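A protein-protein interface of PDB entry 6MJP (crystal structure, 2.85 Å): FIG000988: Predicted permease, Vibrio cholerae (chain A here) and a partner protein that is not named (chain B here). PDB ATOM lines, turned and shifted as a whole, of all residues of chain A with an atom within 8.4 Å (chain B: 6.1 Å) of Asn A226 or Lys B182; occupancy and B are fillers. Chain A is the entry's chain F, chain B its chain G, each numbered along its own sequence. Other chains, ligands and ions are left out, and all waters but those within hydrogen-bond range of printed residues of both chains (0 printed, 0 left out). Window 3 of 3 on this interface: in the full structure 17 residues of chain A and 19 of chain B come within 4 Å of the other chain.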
ATOM      1  N   ASN A 171     -15.239  13.899  -4.102  1.00  0.00           N
ATOM      2  CA  ASN A 171     -14.843  12.598  -4.639  1.00  0.00           C
ATOM      3  C   ASN A 171     -15.115  12.545  -6.148  1.00  0.00           C
ATOM      4  O   ASN A 171     -15.916  11.745  -6.639  1.00  0.00           O
ATOM      5  CB  ASN A 171     -15.561  11.456  -3.892  1.00  0.00           C
ATOM      6  CG  ASN A 171     -14.813  10.155  -3.916  1.00  0.00           C
ATOM      7  OD1 ASN A 171     -13.583  10.136  -3.864  1.00  0.00           O
ATOM      8  ND2 ASN A 171     -15.553   9.049  -3.999  1.00  0.00           N
ATOM      9  N   PHE A 189      -8.798  11.334 -10.975  1.00  0.00           N
ATOM     10  CA  PHE A 189      -9.638  11.114  -9.807  1.00  0.00           C
ATOM     11  C   PHE A 189      -9.055  11.881  -8.633  1.00  0.00           C
ATOM     12  O   PHE A 189      -7.875  11.719  -8.309  1.00  0.00           O
ATOM     13  CB  PHE A 189      -9.727   9.629  -9.456  1.00  0.00           C
ATOM     14  CG  PHE A 189     -10.788   9.315  -8.444  1.00  0.00           C
ATOM     15  CD1 PHE A 189     -12.086   9.076  -8.851  1.00  0.00           C
ATOM     16  CD2 PHE A 189     -10.495   9.265  -7.088  1.00  0.00           C
ATOM     17  CE1 PHE A 189     -13.073   8.791  -7.935  1.00  0.00           C
ATOM     18  CE2 PHE A 189     -11.486   8.981  -6.165  1.00  0.00           C
ATOM     19  CZ  PHE A 189     -12.776   8.742  -6.595  1.00  0.00           C
ATOM     20  N   SER A 190      -9.881  12.697  -7.984  1.00  0.00           N
ATOM     21  CA  SER A 190      -9.404  13.496  -6.863  1.00  0.00           C
ATOM     22  C   SER A 190     -10.305  13.322  -5.645  1.00  0.00           C
ATOM     23  O   SER A 190     -11.168  12.437  -5.618  1.00  0.00           O
ATOM     24  CB  SER A 190      -9.315  14.966  -7.263  1.00  0.00           C
ATOM     25  OG  SER A 190     -10.602  15.512  -7.464  1.00  0.00           O
ATOM     26  N   HIS A 191     -10.105  14.140  -4.620  1.00  0.00           N
ATOM     27  CA  HIS A 191     -10.931  14.047  -3.428  1.00  0.00           C
ATOM     28  C   HIS A 191     -11.982  15.150  -3.366  1.00  0.00           C
ATOM     29  O   HIS A 191     -13.099  14.907  -2.904  1.00  0.00           O
ATOM     30  CB  HIS A 191     -10.049  14.070  -2.169  1.00  0.00           C
ATOM     31  CG  HIS A 191      -9.454  12.737  -1.806  1.00  0.00           C
ATOM     32  ND1 HIS A 191      -8.142  12.404  -2.076  1.00  0.00           N
ATOM     33  CD2 HIS A 191      -9.991  11.663  -1.181  1.00  0.00           C
ATOM     34  CE1 HIS A 191      -7.901  11.179  -1.638  1.00  0.00           C
ATOM     35  NE2 HIS A 191      -9.007  10.708  -1.090  1.00  0.00           N
ATOM     36  N   ASP A 209      -6.203  17.499  -4.401  1.00  0.00           N
ATOM     37  CA  ASP A 209      -5.754  16.233  -3.828  1.00  0.00           C
ATOM     38  C   ASP A 209      -6.172  15.026  -4.665  1.00  0.00           C
ATOM     39  O   ASP A 209      -7.050  14.261  -4.252  1.00  0.00           O
ATOM     40  CB  ASP A 209      -6.291  16.077  -2.393  1.00  0.00           C
ATOM     41  CG  ASP A 209      -5.519  15.032  -1.571  1.00  0.00           C
ATOM     42  OD1 ASP A 209      -4.596  14.373  -2.108  1.00  0.00           O
ATOM     43  OD2 ASP A 209      -5.825  14.883  -0.364  1.00  0.00           O
ATOM     44  N   GLY A 210      -5.556  14.835  -5.825  1.00  0.00           N
ATOM     45  CA  GLY A 210      -5.844  13.668  -6.627  1.00  0.00           C
ATOM     46  C   GLY A 210      -4.665  13.255  -7.484  1.00  0.00           C
ATOM     47  O   GLY A 210      -3.540  13.728  -7.299  1.00  0.00           O
ATOM     48  N   THR A 211      -4.935  12.347  -8.422  1.00  0.00           N
ATOM     49  CA  THR A 211      -3.950  11.895  -9.398  1.00  0.00           C
ATOM     50  C   THR A 211      -4.618  11.822 -10.766  1.00  0.00           C
ATOM     51  O   THR A 211      -5.786  11.433 -10.872  1.00  0.00           O
ATOM     52  CB  THR A 211      -3.349  10.530  -9.004  1.00  0.00           C
ATOM     53  OG1 THR A 211      -4.402   9.604  -8.716  1.00  0.00           O
ATOM     54  CG2 THR A 211      -2.506  10.670  -7.765  1.00  0.00           C
ATOM     55  N   ARG A 212      -3.897  12.238 -11.805  1.00  0.00           N
ATOM     56  CA  ARG A 212      -4.375  12.162 -13.179  1.00  0.00           C
ATOM     57  C   ARG A 212      -3.589  11.101 -13.934  1.00  0.00           C
ATOM     58  O   ARG A 212      -2.368  11.014 -13.787  1.00  0.00           O
ATOM     59  CB  ARG A 212      -4.234  13.509 -13.889  1.00  0.00           C
ATOM     60  CG  ARG A 212      -4.308  13.403 -15.391  1.00  0.00           C
ATOM     61  CD  ARG A 212      -4.520  14.747 -16.034  1.00  0.00           C
ATOM     62  NE  ARG A 212      -4.708  14.612 -17.472  1.00  0.00           N
ATOM     63  CZ  ARG A 212      -5.090  15.598 -18.274  1.00  0.00           C
ATOM     64  NH1 ARG A 212      -5.332  16.802 -17.777  1.00  0.00           N
ATOM     65  NH2 ARG A 212      -5.230  15.378 -19.571  1.00  0.00           N
ATOM     66  N   TYR A 213      -4.285  10.293 -14.736  1.00  0.00           N
ATOM     67  CA  TYR A 213      -3.681   9.178 -15.468  1.00  0.00           C
ATOM     68  C   TYR A 213      -3.897   9.399 -16.961  1.00  0.00           C
ATOM     69  O   TYR A 213      -5.016   9.238 -17.456  1.00  0.00           O
ATOM     70  CB  TYR A 213      -4.275   7.839 -15.017  1.00  0.00           C
ATOM     71  CG  TYR A 213      -4.244   7.626 -13.512  1.00  0.00           C
ATOM     72  CD1 TYR A 213      -5.230   8.159 -12.693  1.00  0.00           C
ATOM     73  CD2 TYR A 213      -3.228   6.893 -12.910  1.00  0.00           C
ATOM     74  CE1 TYR A 213      -5.203   7.974 -11.319  1.00  0.00           C
ATOM     75  CE2 TYR A 213      -3.192   6.705 -11.538  1.00  0.00           C
ATOM     76  CZ  TYR A 213      -4.179   7.244 -10.748  1.00  0.00           C
ATOM     77  OH  TYR A 213      -4.146   7.058  -9.385  1.00  0.00           O
ATOM     78  N   MET A 223       1.253   8.731 -18.166  1.00  0.00           N
ATOM     79  CA  MET A 223       1.831   9.858 -17.447  1.00  0.00           C
ATOM     80  C   MET A 223       0.930  10.151 -16.258  1.00  0.00           C
ATOM     81  O   MET A 223      -0.246  10.478 -16.433  1.00  0.00           O
ATOM     82  CB  MET A 223       1.989  11.097 -18.330  1.00  0.00           C
ATOM     83  CG  MET A 223       2.935  12.125 -17.726  1.00  0.00           C
ATOM     84  SD  MET A 223       2.540  13.827 -18.161  1.00  0.00           S
ATOM     85  CE  MET A 223       2.735  13.783 -19.941  1.00  0.00           C
ATOM     86  N   ILE A 224       1.479  10.021 -15.057  1.00  0.00           N
ATOM     87  CA  ILE A 224       0.733  10.180 -13.819  1.00  0.00           C
ATOM     88  C   ILE A 224       1.090  11.535 -13.236  1.00  0.00           C
ATOM     89  O   ILE A 224       2.271  11.840 -13.036  1.00  0.00           O
ATOM     90  CB  ILE A 224       1.044   9.051 -12.826  1.00  0.00           C
ATOM     91  CG1 ILE A 224       1.137   7.709 -13.552  1.00  0.00           C
ATOM     92  CG2 ILE A 224      -0.019   8.990 -11.750  1.00  0.00           C
ATOM     93  CD1 ILE A 224      -0.126   7.326 -14.279  1.00  0.00           C
ATOM     94  N   THR A 225       0.080  12.345 -12.958  1.00  0.00           N
ATOM     95  CA  THR A 225       0.272  13.661 -12.361  1.00  0.00           C
ATOM     96  C   THR A 225      -0.384  13.650 -10.987  1.00  0.00           C
ATOM     97  O   THR A 225      -1.614  13.619 -10.891  1.00  0.00           O
ATOM     98  CB  THR A 225      -0.330  14.757 -13.246  1.00  0.00           C
ATOM     99  OG1 THR A 225      -0.081  14.463 -14.629  1.00  0.00           O
ATOM    100  CG2 THR A 225       0.271  16.114 -12.902  1.00  0.00           C
ATOM    101  N   ASN A 226       0.425  13.658  -9.927  1.00  0.00           N
ATOM    102  CA  ASN A 226      -0.083  13.804  -8.568  1.00  0.00           C
ATOM    103  C   ASN A 226      -0.176  15.293  -8.271  1.00  0.00           C
ATOM    104  O   ASN A 226       0.842  15.991  -8.234  1.00  0.00           O
ATOM    105  CB  ASN A 226       0.808  13.094  -7.554  1.00  0.00           C
ATOM    106  CG  ASN A 226       0.771  11.591  -7.701  1.00  0.00           C
ATOM    107  OD1 ASN A 226       0.362  11.075  -8.736  1.00  0.00           O
ATOM    108  ND2 ASN A 226       1.204  10.879  -6.667  1.00  0.00           N
ATOM    109  N   PHE A 227      -1.395  15.780  -8.065  1.00  0.00           N
ATOM    110  CA  PHE A 227      -1.658  17.204  -7.949  1.00  0.00           C
ATOM    111  C   PHE A 227      -2.311  17.508  -6.610  1.00  0.00           C
ATOM    112  O   PHE A 227      -3.157  16.745  -6.133  1.00  0.00           O
ATOM    113  CB  PHE A 227      -2.558  17.703  -9.103  1.00  0.00           C
ATOM    114  CG  PHE A 227      -3.833  16.914  -9.281  1.00  0.00           C
ATOM    115  CD1 PHE A 227      -4.977  17.238  -8.565  1.00  0.00           C
ATOM    116  CD2 PHE A 227      -3.891  15.862 -10.180  1.00  0.00           C
ATOM    117  CE1 PHE A 227      -6.146  16.515  -8.732  1.00  0.00           C
ATOM    118  CE2 PHE A 227      -5.059  15.140 -10.351  1.00  0.00           C
ATOM    119  CZ  PHE A 227      -6.186  15.468  -9.627  1.00  0.00           C
ATOM    120  N   ASP A 228      -1.894  18.615  -5.995  1.00  0.00           N
ATOM    121  CA  ASP A 228      -2.681  19.180  -4.907  1.00  0.00           C
ATOM    122  C   ASP A 228      -3.788  20.064  -5.462  1.00  0.00           C
ATOM    123  O   ASP A 228      -4.896  20.096  -4.914  1.00  0.00           O
ATOM    124  CB  ASP A 228      -1.787  19.971  -3.948  1.00  0.00           C
ATOM    125  CG  ASP A 228      -0.716  19.106  -3.285  1.00  0.00           C
ATOM    126  OD1 ASP A 228      -0.902  17.873  -3.180  1.00  0.00           O
ATOM    127  OD2 ASP A 228       0.315  19.671  -2.857  1.00  0.00           O
ATOM    128  N   SER A 229      -3.510  20.767  -6.560  1.00  0.00           N
ATOM    129  CA  SER A 229      -4.488  21.603  -7.247  1.00  0.00           C
ATOM    130  C   SER A 229      -4.274  21.488  -8.750  1.00  0.00           C
ATOM    131  O   SER A 229      -3.134  21.557  -9.222  1.00  0.00           O
ATOM    132  CB  SER A 229      -4.374  23.066  -6.806  1.00  0.00           C
ATOM    133  OG  SER A 229      -5.273  23.884  -7.533  1.00  0.00           O
ATOM    134  N   TYR A 230      -5.371  21.317  -9.490  1.00  0.00           N
ATOM    135  CA  TYR A 230      -5.318  21.180 -10.942  1.00  0.00           C
ATOM    136  C   TYR A 230      -6.606  21.724 -11.548  1.00  0.00           C
ATOM    137  O   TYR A 230      -7.699  21.392 -11.082  1.00  0.00           O
ATOM    138  CB  TYR A 230      -5.112  19.715 -11.353  1.00  0.00           C
ATOM    139  N   ARG B 176     -10.372   0.336 -11.801  1.00  0.00           N
ATOM    140  CA  ARG B 176     -10.542   0.057 -10.380  1.00  0.00           C
ATOM    141  C   ARG B 176      -9.746   1.047  -9.543  1.00  0.00           C
ATOM    142  O   ARG B 176      -8.625   1.415  -9.904  1.00  0.00           O
ATOM    143  CB  ARG B 176     -10.107  -1.368 -10.028  1.00  0.00           C
ATOM    144  CG  ARG B 176     -11.158  -2.428 -10.327  1.00  0.00           C
ATOM    145  CD  ARG B 176     -11.072  -3.604  -9.361  1.00  0.00           C
ATOM    146  NE  ARG B 176     -12.259  -4.454  -9.440  1.00  0.00           N
ATOM    147  CZ  ARG B 176     -12.331  -5.581 -10.141  1.00  0.00           C
ATOM    148  NH1 ARG B 176     -11.278  -6.006 -10.822  1.00  0.00           N
ATOM    149  NH2 ARG B 176     -13.455  -6.289 -10.157  1.00  0.00           N
ATOM    150  N   PHE B 177     -10.319   1.463  -8.414  1.00  0.00           N
ATOM    151  CA  PHE B 177      -9.638   2.355  -7.485  1.00  0.00           C
ATOM    152  C   PHE B 177      -9.630   1.758  -6.081  1.00  0.00           C
ATOM    153  O   PHE B 177     -10.594   1.106  -5.665  1.00  0.00           O
ATOM    154  CB  PHE B 177     -10.288   3.740  -7.489  1.00  0.00           C
ATOM    155  CG  PHE B 177     -10.114   4.480  -8.786  1.00  0.00           C
ATOM    156  CD1 PHE B 177     -10.934   4.213  -9.872  1.00  0.00           C
ATOM    157  CD2 PHE B 177      -9.116   5.430  -8.928  1.00  0.00           C
ATOM    158  CE1 PHE B 177     -10.766   4.889 -11.074  1.00  0.00           C
ATOM    159  CE2 PHE B 177      -8.944   6.108 -10.121  1.00  0.00           C
ATOM    160  CZ  PHE B 177      -9.769   5.837 -11.197  1.00  0.00           C
ATOM    161  N   ASP B 178      -8.529   1.976  -5.361  1.00  0.00           N
ATOM    162  CA  ASP B 178      -8.327   1.403  -4.040  1.00  0.00           C
ATOM    163  C   ASP B 178      -8.897   2.324  -2.963  1.00  0.00           C
ATOM    164  O   ASP B 178      -9.513   3.354  -3.249  1.00  0.00           O
ATOM    165  CB  ASP B 178      -6.842   1.132  -3.796  1.00  0.00           C
ATOM    166  CG  ASP B 178      -6.015   2.405  -3.721  1.00  0.00           C
ATOM    167  OD1 ASP B 178      -6.428   3.423  -4.315  1.00  0.00           O
ATOM    168  OD2 ASP B 178      -4.947   2.388  -3.072  1.00  0.00           O
ATOM    169  N   GLU B 179      -8.682   1.948  -1.698  1.00  0.00           N
ATOM    170  CA  GLU B 179      -9.159   2.768  -0.590  1.00  0.00           C
ATOM    171  C   GLU B 179      -8.482   4.131  -0.562  1.00  0.00           C
ATOM    172  O   GLU B 179      -9.048   5.087  -0.016  1.00  0.00           O
ATOM    173  CB  GLU B 179      -8.939   2.040   0.737  1.00  0.00           C
ATOM    174  CG  GLU B 179      -9.706   2.632   1.915  1.00  0.00           C
ATOM    175  N   ASN B 180      -7.296   4.246  -1.149  1.00  0.00           N
ATOM    176  CA  ASN B 180      -6.579   5.510  -1.248  1.00  0.00           C
ATOM    177  C   ASN B 180      -7.023   6.355  -2.433  1.00  0.00           C
ATOM    178  O   ASN B 180      -6.363   7.355  -2.735  1.00  0.00           O
ATOM    179  CB  ASN B 180      -5.076   5.253  -1.347  1.00  0.00           C
ATOM    180  CG  ASN B 180      -4.459   4.919  -0.019  1.00  0.00           C
ATOM    181  OD1 ASN B 180      -5.159   4.647   0.959  1.00  0.00           O
ATOM    182  ND2 ASN B 180      -3.138   4.939   0.029  1.00  0.00           N
ATOM    183  N   LYS B 181      -8.096   5.953  -3.117  1.00  0.00           N
ATOM    184  CA  LYS B 181      -8.686   6.721  -4.219  1.00  0.00           C
ATOM    185  C   LYS B 181      -7.701   6.904  -5.378  1.00  0.00           C
ATOM    186  O   LYS B 181      -7.668   7.955  -6.028  1.00  0.00           O
ATOM    187  CB  LYS B 181      -9.209   8.070  -3.728  1.00  0.00           C
ATOM    188  N   LYS B 182      -6.908   5.857  -5.656  1.00  0.00           N
ATOM    189  CA  LYS B 182      -5.949   5.837  -6.751  1.00  0.00           C
ATOM    190  C   LYS B 182      -6.129   4.576  -7.586  1.00  0.00           C
ATOM    191  O   LYS B 182      -6.640   3.566  -7.105  1.00  0.00           O
ATOM    192  CB  LYS B 182      -4.489   5.933  -6.238  1.00  0.00           C
ATOM    193  CG  LYS B 182      -4.167   7.243  -5.533  1.00  0.00           C
ATOM    194  CD  LYS B 182      -2.733   7.284  -4.999  1.00  0.00           C
ATOM    195  CE  LYS B 182      -1.700   7.407  -6.115  1.00  0.00           C
ATOM    196  NZ  LYS B 182      -0.312   7.590  -5.583  1.00  0.00           N
ATOM    197  N   LEU B 183      -5.713   4.651  -8.847  1.00  0.00           N
ATOM    198  CA  LEU B 183      -6.121   3.679  -9.842  1.00  0.00           C
ATOM    199  C   LEU B 183      -5.180   2.489  -9.766  1.00  0.00           C
ATOM    200  O   LEU B 183      -3.978   2.622  -9.977  1.00  0.00           O
ATOM    201  CB  LEU B 183      -6.133   4.348 -11.212  1.00  0.00           C
ATOM    202  CG  LEU B 183      -6.208   3.433 -12.440  1.00  0.00           C
ATOM    203  CD1 LEU B 183      -7.591   2.819 -12.616  1.00  0.00           C
ATOM    204  CD2 LEU B 183      -5.759   4.122 -13.745  1.00  0.00           C
ATOM    205  N   SER B 184      -5.726   1.311  -9.511  1.00  0.00           N
ATOM    206  CA  SER B 184      -4.909   0.118  -9.335  1.00  0.00           C
ATOM    207  C   SER B 184      -4.872  -0.750 -10.590  1.00  0.00           C
ATOM    208  O   SER B 184      -3.789  -1.147 -11.036  1.00  0.00           O
ATOM    209  CB  SER B 184      -5.407  -0.678  -8.137  1.00  0.00           C
ATOM    210  OG  SER B 184      -6.752  -1.106  -8.335  1.00  0.00           O
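The side-chain hydroxyl (OH) of Tyr A213 sits at hydrogen-bond distance from the backbone NH (N) of Leu B183.
O of Asp A209 sits at hydrogen-bond distance from ND1 of His A191, 3.1 Å away.
The backbone carbonyl oxygen (O) of His A191 sits at hydrogen-bond distance from the backbone NH (N) of Asn A171, 2.7 Å away.
The backbone NH of Lys B181 lies within hydrogen-bond range of the side-chain carboxylate of Asp B178, at 3.3 Å.
The backbone NH (N) of Thr A211 sits at hydrogen-bond distance from the backbone carbonyl oxygen (O) of Phe A189 (3.0 Å).
The side-chain hydroxyl (OG1) of Thr A211 lies within hydrogen-bond range of the side-chain hydroxyl (OH) of Tyr A213 (2.6 Å).
OD1 of Asp B178 lies within hydrogen-bond range of N of Lys B182, at 2.8 Å.
Among the printed residues, merely in contact across the chains: Phe A189 with Lys B181, Tyr A213 with Lys B182, Phe A189 with Phe B177, His A191 with Lys B181, Thr A211 with Lys B182 and Asn A226 with Lys B182.
Of the printed residues of chain B, Phe A189 touches Phe B177 (3.7 Å) and Lys B181 (3.3 Å).
Printed residues of chain B within 4 Å of Tyr A213: Lys B182 (3.4 Å) and Leu B183 (2.9 Å).
Asn A226 touches just one residue of chain B: Lys B182 (3.8 Å).
Of the printed residues of chain A, Phe B177 touches Phe A189 (3.7 Å).
Lys B181 touches just these residues of chain A: Phe A189 (3.3 Å) and His A191 (3.7 Å).
Lys B182 touches just these residues of chain A: Thr A211, Tyr A213 and Asn A226.
Of the printed residues of chain A, Leu B183 touches Tyr A213.
The nearest residue of chain A that does not touch Lys B182 is Phe A189 (5.2 Å).
The nearest printed residue of chain A that does not touch Leu B183 is Thr A211 (5.1 Å).
Hydrophobic or aromatic side chains of chain B within 4 Å of the printed part of chain A: Phe B177 and Leu B183.
Along chain B the printed residues that touch a printed residue of chain A span positions 177 to 183.
Hydrophobic or aromatic side chains of chain A that line the printed part of chain B: Phe A189, His A191 and Tyr A213.
Among the printed residues, no Asp or Glu carboxylate lies within 4 Å of a Lys or Arg side-chain nitrogen of the other chain.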
